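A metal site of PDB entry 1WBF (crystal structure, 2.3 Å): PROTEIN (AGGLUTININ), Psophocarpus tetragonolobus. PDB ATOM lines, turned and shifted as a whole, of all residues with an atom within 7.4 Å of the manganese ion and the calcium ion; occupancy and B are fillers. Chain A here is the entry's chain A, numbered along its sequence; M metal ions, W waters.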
ATOM      1  N   ASP A  88      29.692 -34.649  30.916  1.00  0.00           N
ATOM      2  CA  ASP A  88      28.865 -33.502  30.503  1.00  0.00           C
ATOM      3  C   ASP A  88      27.930 -32.977  31.575  1.00  0.00           C
ATOM      4  O   ASP A  88      27.669 -31.774  31.626  1.00  0.00           O
ATOM      5  CB  ASP A  88      28.035 -33.860  29.266  1.00  0.00           C
ATOM      6  CG  ASP A  88      28.756 -33.528  27.966  1.00  0.00           C
ATOM      7  OD1 ASP A  88      28.852 -32.338  27.606  1.00  0.00           O
ATOM      8  OD2 ASP A  88      29.243 -34.455  27.315  1.00  0.00           O
ATOM      9  N   GLY A  89      27.426 -33.863  32.437  1.00  0.00           N
ATOM     10  CA  GLY A  89      26.549 -33.450  33.520  1.00  0.00           C
ATOM     11  C   GLY A  89      25.430 -34.450  33.773  1.00  0.00           C
ATOM     12  O   GLY A  89      25.390 -35.498  33.127  1.00  0.00           O
ATOM     13  N   GLY A 105      26.268 -36.703  25.508  1.00  0.00           N
ATOM     14  CA  GLY A 105      26.956 -35.433  25.471  1.00  0.00           C
ATOM     15  C   GLY A 105      26.193 -34.334  26.182  1.00  0.00           C
ATOM     16  O   GLY A 105      25.659 -34.534  27.275  1.00  0.00           O
ATOM     17  N   GLY A 106      26.123 -33.166  25.550  1.00  0.00           N
ATOM     18  CA  GLY A 106      25.412 -32.031  26.131  1.00  0.00           C
ATOM     19  C   GLY A 106      23.901 -32.171  26.125  1.00  0.00           C
ATOM     20  O   GLY A 106      23.225 -31.195  26.387  1.00  0.00           O
ATOM     21  N   TYR A 107      23.389 -33.350  25.751  1.00  0.00           N
ATOM     22  CA  TYR A 107      21.945 -33.639  25.738  1.00  0.00           C
ATOM     23  C   TYR A 107      21.567 -34.509  26.920  1.00  0.00           C
ATOM     24  O   TYR A 107      20.389 -34.829  27.105  1.00  0.00           O
ATOM     25  CB  TYR A 107      21.540 -34.382  24.463  1.00  0.00           C
ATOM     26  CG  TYR A 107      21.608 -33.547  23.201  1.00  0.00           C
ATOM     27  CD1 TYR A 107      21.650 -32.161  23.260  1.00  0.00           C
ATOM     28  CD2 TYR A 107      21.652 -34.159  21.958  1.00  0.00           C
ATOM     29  CE1 TYR A 107      21.749 -31.399  22.104  1.00  0.00           C
ATOM     30  CE2 TYR A 107      21.753 -33.403  20.796  1.00  0.00           C
ATOM     31  CZ  TYR A 107      21.794 -32.031  20.881  1.00  0.00           C
ATOM     32  OH  TYR A 107      21.887 -31.275  19.730  1.00  0.00           O
ATOM     33  N   PHE A 108      22.592 -35.024  27.618  1.00  0.00           N
ATOM     34  CA  PHE A 108      22.409 -35.835  28.834  1.00  0.00           C
ATOM     35  C   PHE A 108      21.713 -37.176  28.697  1.00  0.00           C
ATOM     36  O   PHE A 108      21.404 -37.824  29.705  1.00  0.00           O
ATOM     37  CB  PHE A 108      21.671 -35.000  29.902  1.00  0.00           C
ATOM     38  CG  PHE A 108      22.205 -33.599  30.073  1.00  0.00           C
ATOM     39  CD1 PHE A 108      23.476 -33.372  30.598  1.00  0.00           C
ATOM     40  CD2 PHE A 108      21.448 -32.505  29.662  1.00  0.00           C
ATOM     41  CE1 PHE A 108      23.982 -32.076  30.705  1.00  0.00           C
ATOM     42  CE2 PHE A 108      21.946 -31.206  29.763  1.00  0.00           C
ATOM     43  CZ  PHE A 108      23.213 -30.991  30.285  1.00  0.00           C
ATOM     44  N   GLU A 123      19.038 -29.439  35.348  1.00  0.00           N
ATOM     45  CA  GLU A 123      20.376 -29.870  35.007  1.00  0.00           C
ATOM     46  C   GLU A 123      21.502 -29.253  35.823  1.00  0.00           C
ATOM     47  O   GLU A 123      21.451 -28.077  36.164  1.00  0.00           O
ATOM     48  CB  GLU A 123      20.670 -29.552  33.529  1.00  0.00           C
ATOM     49  CG  GLU A 123      20.748 -28.056  33.282  1.00  0.00           C
ATOM     50  CD  GLU A 123      21.148 -27.688  31.876  1.00  0.00           C
ATOM     51  OE1 GLU A 123      20.616 -28.279  30.911  1.00  0.00           O
ATOM     52  OE2 GLU A 123      21.955 -26.772  31.759  1.00  0.00           O
ATOM     53  N   PHE A 124      22.532 -30.052  36.057  1.00  0.00           N
ATOM     54  CA  PHE A 124      23.738 -29.647  36.760  1.00  0.00           C
ATOM     55  C   PHE A 124      24.735 -29.967  35.670  1.00  0.00           C
ATOM     56  O   PHE A 124      25.061 -31.141  35.399  1.00  0.00           O
ATOM     57  CB  PHE A 124      23.917 -30.487  38.034  1.00  0.00           C
ATOM     58  CG  PHE A 124      22.751 -30.390  38.972  1.00  0.00           C
ATOM     59  CD1 PHE A 124      22.682 -29.378  39.927  1.00  0.00           C
ATOM     60  CD2 PHE A 124      21.684 -31.285  38.860  1.00  0.00           C
ATOM     61  CE1 PHE A 124      21.577 -29.268  40.760  1.00  0.00           C
ATOM     62  CE2 PHE A 124      20.561 -31.192  39.688  1.00  0.00           C
ATOM     63  CZ  PHE A 124      20.508 -30.183  40.638  1.00  0.00           C
ATOM     64  N   ASP A 125      25.047 -28.899  34.941  1.00  0.00           N
ATOM     65  CA  ASP A 125      25.885 -28.879  33.747  1.00  0.00           C
ATOM     66  C   ASP A 125      27.333 -28.475  33.950  1.00  0.00           C
ATOM     67  O   ASP A 125      27.634 -27.348  34.349  1.00  0.00           O
ATOM     68  CB  ASP A 125      25.232 -27.914  32.756  1.00  0.00           C
ATOM     69  CG  ASP A 125      25.615 -28.186  31.314  1.00  0.00           C
ATOM     70  OD1 ASP A 125      26.819 -28.244  31.014  1.00  0.00           O
ATOM     71  OD2 ASP A 125      24.699 -28.337  30.490  1.00  0.00           O
ATOM     72  N   THR A 126      28.224 -29.340  33.467  1.00  0.00           N
ATOM     73  CA  THR A 126      29.661 -29.172  33.621  1.00  0.00           C
ATOM     74  C   THR A 126      30.455 -28.867  32.369  1.00  0.00           C
ATOM     75  O   THR A 126      31.655 -28.600  32.453  1.00  0.00           O
ATOM     76  CB  THR A 126      30.255 -30.403  34.294  1.00  0.00           C
ATOM     77  OG1 THR A 126      29.971 -31.561  33.506  1.00  0.00           O
ATOM     78  CG2 THR A 126      29.626 -30.592  35.671  1.00  0.00           C
ATOM     79  N   PHE A 127      29.820 -28.879  31.206  1.00  0.00           N
ATOM     80  CA  PHE A 127      30.530 -28.594  29.961  1.00  0.00           C
ATOM     81  C   PHE A 127      29.878 -27.428  29.217  1.00  0.00           C
ATOM     82  O   PHE A 127      28.665 -27.419  29.011  1.00  0.00           O
ATOM     83  CB  PHE A 127      30.565 -29.843  29.091  1.00  0.00           C
ATOM     84  CG  PHE A 127      31.322 -29.666  27.822  1.00  0.00           C
ATOM     85  CD1 PHE A 127      32.642 -29.269  27.835  1.00  0.00           C
ATOM     86  CD2 PHE A 127      30.709 -29.931  26.609  1.00  0.00           C
ATOM     87  CE1 PHE A 127      33.351 -29.129  26.656  1.00  0.00           C
ATOM     88  CE2 PHE A 127      31.399 -29.800  25.432  1.00  0.00           C
ATOM     89  CZ  PHE A 127      32.732 -29.400  25.447  1.00  0.00           C
ATOM     90  N   ARG A 128      30.649 -26.421  28.820  1.00  0.00           N
ATOM     91  CA  ARG A 128      30.051 -25.270  28.137  1.00  0.00           C
ATOM     92  C   ARG A 128      29.927 -25.364  26.619  1.00  0.00           C
ATOM     93  O   ARG A 128      30.867 -25.022  25.901  1.00  0.00           O
ATOM     94  CB  ARG A 128      30.768 -23.974  28.479  1.00  0.00           C
ATOM     95  CG  ARG A 128      29.845 -22.793  28.385  1.00  0.00           C
ATOM     96  CD  ARG A 128      30.418 -21.720  27.537  1.00  0.00           C
ATOM     97  NE  ARG A 128      30.830 -20.590  28.335  1.00  0.00           N
ATOM     98  CZ  ARG A 128      30.375 -19.345  28.173  1.00  0.00           C
ATOM     99  NH1 ARG A 128      29.488 -19.076  27.230  1.00  0.00           N
ATOM    100  NH2 ARG A 128      30.838 -18.367  28.933  1.00  0.00           N
ATOM    101  N   ASN A 129      28.760 -25.813  26.153  1.00  0.00           N
ATOM    102  CA  ASN A 129      28.472 -25.904  24.723  1.00  0.00           C
ATOM    103  C   ASN A 129      28.220 -24.510  24.187  1.00  0.00           C
ATOM    104  O   ASN A 129      28.223 -23.549  24.931  1.00  0.00           O
ATOM    105  CB  ASN A 129      27.237 -26.742  24.461  1.00  0.00           C
ATOM    106  CG  ASN A 129      27.407 -28.156  24.863  1.00  0.00           C
ATOM    107  OD1 ASN A 129      27.207 -28.498  26.013  1.00  0.00           O
ATOM    108  ND2 ASN A 129      27.720 -29.010  23.906  1.00  0.00           N
ATOM    109  N   THR A 130      27.949 -24.410  22.892  1.00  0.00           N
ATOM    110  CA  THR A 130      27.702 -23.099  22.281  1.00  0.00           C
ATOM    111  C   THR A 130      26.432 -22.438  22.822  1.00  0.00           C
ATOM    112  O   THR A 130      26.374 -21.213  22.959  1.00  0.00           O
ATOM    113  CB  THR A 130      27.647 -23.192  20.728  1.00  0.00           C
ATOM    114  OG1 THR A 130      26.748 -24.244  20.337  1.00  0.00           O
ATOM    115  CG2 THR A 130      29.037 -23.497  20.156  1.00  0.00           C
ATOM    116  N   TRP A 131      25.452 -23.267  23.197  1.00  0.00           N
ATOM    117  CA  TRP A 131      24.173 -22.795  23.717  1.00  0.00           C
ATOM    118  C   TRP A 131      24.150 -22.693  25.236  1.00  0.00           C
ATOM    119  O   TRP A 131      23.079 -22.686  25.838  1.00  0.00           O
ATOM    120  CB  TRP A 131      23.090 -23.804  23.326  1.00  0.00           C
ATOM    121  CG  TRP A 131      23.274 -25.150  23.979  1.00  0.00           C
ATOM    122  CD1 TRP A 131      23.065 -25.473  25.291  1.00  0.00           C
ATOM    123  CD2 TRP A 131      23.687 -26.347  23.321  1.00  0.00           C
ATOM    124  NE1 TRP A 131      23.314 -26.798  25.492  1.00  0.00           N
ATOM    125  CE2 TRP A 131      23.699 -27.373  24.308  1.00  0.00           C
ATOM    126  CE3 TRP A 131      24.050 -26.677  22.024  1.00  0.00           C
ATOM    127  CZ2 TRP A 131      24.057 -28.687  24.011  1.00  0.00           C
ATOM    128  CZ3 TRP A 131      24.400 -27.987  21.722  1.00  0.00           C
ATOM    129  CH2 TRP A 131      24.395 -28.972  22.722  1.00  0.00           C
ATOM    130  N   ASP A 132      25.322 -22.636  25.849  1.00  0.00           N
ATOM    131  CA  ASP A 132      25.445 -22.602  27.295  1.00  0.00           C
ATOM    132  C   ASP A 132      26.141 -21.400  27.847  1.00  0.00           C
ATOM    133  O   ASP A 132      26.951 -20.793  27.148  1.00  0.00           O
ATOM    134  CB  ASP A 132      26.293 -23.773  27.752  1.00  0.00           C
ATOM    135  CG  ASP A 132      25.488 -24.908  28.162  1.00  0.00           C
ATOM    136  OD1 ASP A 132      24.464 -24.664  28.821  1.00  0.00           O
ATOM    137  OD2 ASP A 132      25.891 -26.031  27.825  1.00  0.00           O
ATOM    138  N   PRO A 133      25.794 -20.970  29.082  1.00  0.00           N
ATOM    139  CA  PRO A 133      26.421 -19.831  29.770  1.00  0.00           C
ATOM    140  C   PRO A 133      27.576 -20.445  30.588  1.00  0.00           C
ATOM    141  O   PRO A 133      27.703 -21.661  30.648  1.00  0.00           O
ATOM    142  CB  PRO A 133      25.305 -19.328  30.693  1.00  0.00           C
ATOM    143  CG  PRO A 133      24.600 -20.570  31.065  1.00  0.00           C
ATOM    144  CD  PRO A 133      24.493 -21.279  29.726  1.00  0.00           C
ATOM    145  N   ILE A 135      30.018 -22.282  32.939  1.00  0.00           N
ATOM    146  CA  ILE A 135      29.829 -23.499  33.748  1.00  0.00           C
ATOM    147  C   ILE A 135      30.691 -23.496  35.033  1.00  0.00           C
ATOM    148  O   ILE A 135      31.664 -22.734  35.129  1.00  0.00           O
ATOM    149  CB  ILE A 135      30.116 -24.804  32.939  1.00  0.00           C
ATOM    150  CG1 ILE A 135      31.454 -24.729  32.204  1.00  0.00           C
ATOM    151  CG2 ILE A 135      28.963 -25.122  32.015  1.00  0.00           C
ATOM    152  CD1 ILE A 135      32.655 -25.132  33.062  1.00  0.00           C
ATOM    153  N   HIS A 137      26.696 -24.747  36.112  1.00  0.00           N
ATOM    154  CA  HIS A 137      25.467 -24.012  36.370  1.00  0.00           C
ATOM    155  C   HIS A 137      24.338 -24.986  36.426  1.00  0.00           C
ATOM    156  O   HIS A 137      24.449 -26.103  35.908  1.00  0.00           O
ATOM    157  CB  HIS A 137      25.172 -22.935  35.288  1.00  0.00           C
ATOM    158  CG  HIS A 137      25.087 -23.461  33.881  1.00  0.00           C
ATOM    159  ND1 HIS A 137      25.973 -23.085  32.887  1.00  0.00           N
ATOM    160  CD2 HIS A 137      24.217 -24.326  33.295  1.00  0.00           C
ATOM    161  CE1 HIS A 137      25.661 -23.692  31.753  1.00  0.00           C
ATOM    162  NE2 HIS A 137      24.598 -24.453  31.982  1.00  0.00           N
ATOM    163  N   ILE A 138      23.306 -24.625  37.186  1.00  0.00           N
ATOM    164  CA  ILE A 138      22.101 -25.434  37.287  1.00  0.00           C
ATOM    165  C   ILE A 138      21.207 -24.780  36.232  1.00  0.00           C
ATOM    166  O   ILE A 138      21.289 -23.563  36.011  1.00  0.00           O
ATOM    167  CB  ILE A 138      21.320 -25.216  38.628  1.00  0.00           C
ATOM    168  CG1 ILE A 138      22.258 -25.152  39.838  1.00  0.00           C
ATOM    169  CG2 ILE A 138      20.261 -26.297  38.822  1.00  0.00           C
ATOM    170  CD1 ILE A 138      21.558 -24.580  41.109  1.00  0.00           C
ATOM    171  N   GLY A 139      20.327 -25.544  35.617  1.00  0.00           N
ATOM    172  CA  GLY A 139      19.428 -24.954  34.649  1.00  0.00           C
ATOM    173  C   GLY A 139      18.080 -25.626  34.619  1.00  0.00           C
ATOM    174  O   GLY A 139      17.975 -26.806  34.910  1.00  0.00           O
ATOM    175  N   ASP A 141      15.134 -26.898  32.350  1.00  0.00           N
ATOM    176  CA  ASP A 141      14.912 -27.183  30.940  1.00  0.00           C
ATOM    177  C   ASP A 141      13.483 -27.596  30.654  1.00  0.00           C
ATOM    178  O   ASP A 141      12.959 -28.477  31.321  1.00  0.00           O
ATOM    179  CB  ASP A 141      15.822 -28.332  30.479  1.00  0.00           C
ATOM    180  CG  ASP A 141      17.278 -28.025  30.662  1.00  0.00           C
ATOM    181  OD1 ASP A 141      17.601 -26.843  30.790  1.00  0.00           O
ATOM    182  OD2 ASP A 141      18.091 -28.964  30.649  1.00  0.00           O
ATOM    183  N   VAL A 145      17.561 -28.237  25.856  1.00  0.00           N
ATOM    184  CA  VAL A 145      18.694 -28.051  26.757  1.00  0.00           C
ATOM    185  C   VAL A 145      19.167 -26.607  26.756  1.00  0.00           C
ATOM    186  O   VAL A 145      20.252 -26.295  27.171  1.00  0.00           O
ATOM    187  CB  VAL A 145      19.909 -28.979  26.465  1.00  0.00           C
ATOM    188  CG1 VAL A 145      19.572 -30.411  26.822  1.00  0.00           C
ATOM    189  CG2 VAL A 145      20.338 -28.870  25.015  1.00  0.00           C
ATOM    190  N   ILE A 146      18.374 -25.710  26.195  1.00  0.00           N
ATOM    191  CA  ILE A 146      18.673 -24.290  26.175  1.00  0.00           C
ATOM    192  C   ILE A 146      17.760 -23.810  27.310  1.00  0.00           C
ATOM    193  O   ILE A 146      16.593 -23.540  27.125  1.00  0.00           O
ATOM    194  CB  ILE A 146      18.326 -23.653  24.829  1.00  0.00           C
ATOM    195  CG1 ILE A 146      18.924 -24.513  23.698  1.00  0.00           C
ATOM    196  CG2 ILE A 146      18.908 -22.236  24.759  1.00  0.00           C
ATOM    197  CD1 ILE A 146      18.462 -24.158  22.285  1.00  0.00           C
ATOM    198  N   SER A 147      18.286 -23.894  28.516  1.00  0.00           N
ATOM    199  CA  SER A 147      17.591 -23.536  29.751  1.00  0.00           C
ATOM    200  C   SER A 147      16.805 -22.247  29.725  1.00  0.00           C
ATOM    201  O   SER A 147      17.233 -21.250  29.115  1.00  0.00           O
ATOM    202  CB  SER A 147      18.581 -23.487  30.920  1.00  0.00           C
ATOM    203  OG  SER A 147      19.356 -24.672  30.973  1.00  0.00           O
ATOM    204  N   THR A 150      19.081 -20.003  34.435  1.00  0.00           N
ATOM    205  CA  THR A 150      20.359 -20.599  34.865  1.00  0.00           C
ATOM    206  C   THR A 150      20.997 -19.831  36.034  1.00  0.00           C
ATOM    207  O   THR A 150      20.759 -18.629  36.193  1.00  0.00           O
ATOM    208  CB  THR A 150      21.468 -20.747  33.759  1.00  0.00           C
ATOM    209  OG1 THR A 150      21.988 -19.465  33.404  1.00  0.00           O
ATOM    210  CG2 THR A 150      20.962 -21.466  32.557  1.00  0.00           C
HETATM  211 MN    MN M   1      23.326 -26.197  30.081  1.00  0.00          MN
HETATM  212 CA    CA M   2      26.488 -28.209  28.519  1.00  0.00          CA
HETATM  213  O   HOH W   1      21.991 -27.364  28.800  1.00  0.00           O
HETATM  214  O   HOH W   2      27.340 -30.398  28.570  1.00  0.00           O
HETATM  215  O   HOH W   3      24.157 -29.330  27.700  1.00  0.00           O
HETATM  216  O   HOH W   4      22.222 -24.062  30.283  1.00  0.00           O
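OE2 of Glu 123 sits close to OG of Ser 147. OD2 of Asp 141 sits close to OE1 of Glu 123, 2.6 Å away. The backbone NH of Gly 139 lies within hydrogen-bond range of the backbone carbonyl oxygen of Glu 123, 2.8 Å away. A ring nitrogen (NE2) of His 137 lies close to the side-chain carboxylate (OD1) of Asp 132, 3.2 Å away. The backbone carbonyl oxygen (O) of Asp 132 lies within hydrogen-bond range of the guanidinium group (NH1) of Arg 128, at 3.1 Å. The backbone NH of Asp 125 lies within hydrogen-bond range of the backbone carbonyl oxygen of His 137. ND1 of His 137 lies close to O of Pro 133 (3.2 Å).
Four residues have an atom within 4 Å of the calcium ion: Asp 125, Phe 127, Asn 129 and Asp 132. Along chain A the residues within 4 Å of the calcium ion span positions 125 to 132.
The calcium ion is bound by water W2, 2.3 Å away. The side-chain carboxylate (OD2) of Asp 132 is bound to the calcium ion, 2.4 Å away. The backbone carbonyl oxygen (O) of Phe 127 is bound to the calcium ion. OD1 of Asp 125 binds the calcium ion (2.5 Å). The calcium ion is bound by OD1 of Asn 129, at 2.6 Å. The calcium ion is bound by OD2 of Asp 125 (2.7 Å). The calcium ion is bound by water W3 (2.7 Å).
The manganese ion is bound by water W1, the side-chain carboxylate of Glu 123, the side-chain carboxylate of Asp 132, water W4 and the side-chain carboxylate of Asp 125. The manganese ion has five donor atoms within binding distance. Slightly farther from the manganese ion lies NE2 of His 137 (2.9 Å).
Water W4 lies within hydrogen-bond range of a ring nitrogen (NE2) of His 137 (2.9 Å) and the side-chain hydroxyl (OG) of Ser 147 (3.0 Å). Water W1 lies within hydrogen-bond range of O of Val 145 (2.6 Å) and OE1 of Glu 123 (2.7 Å). Water W3 lies within hydrogen-bond range of the backbone carbonyl oxygen of Gly 106 and the indole nitrogen of Trp 131.
Within 4 Å of the manganese ion: Glu 123, Asp 125, Asp 132 and His 137. The nearest printed residue that does not touch the manganese ion is Val 145 (4.2 Å).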
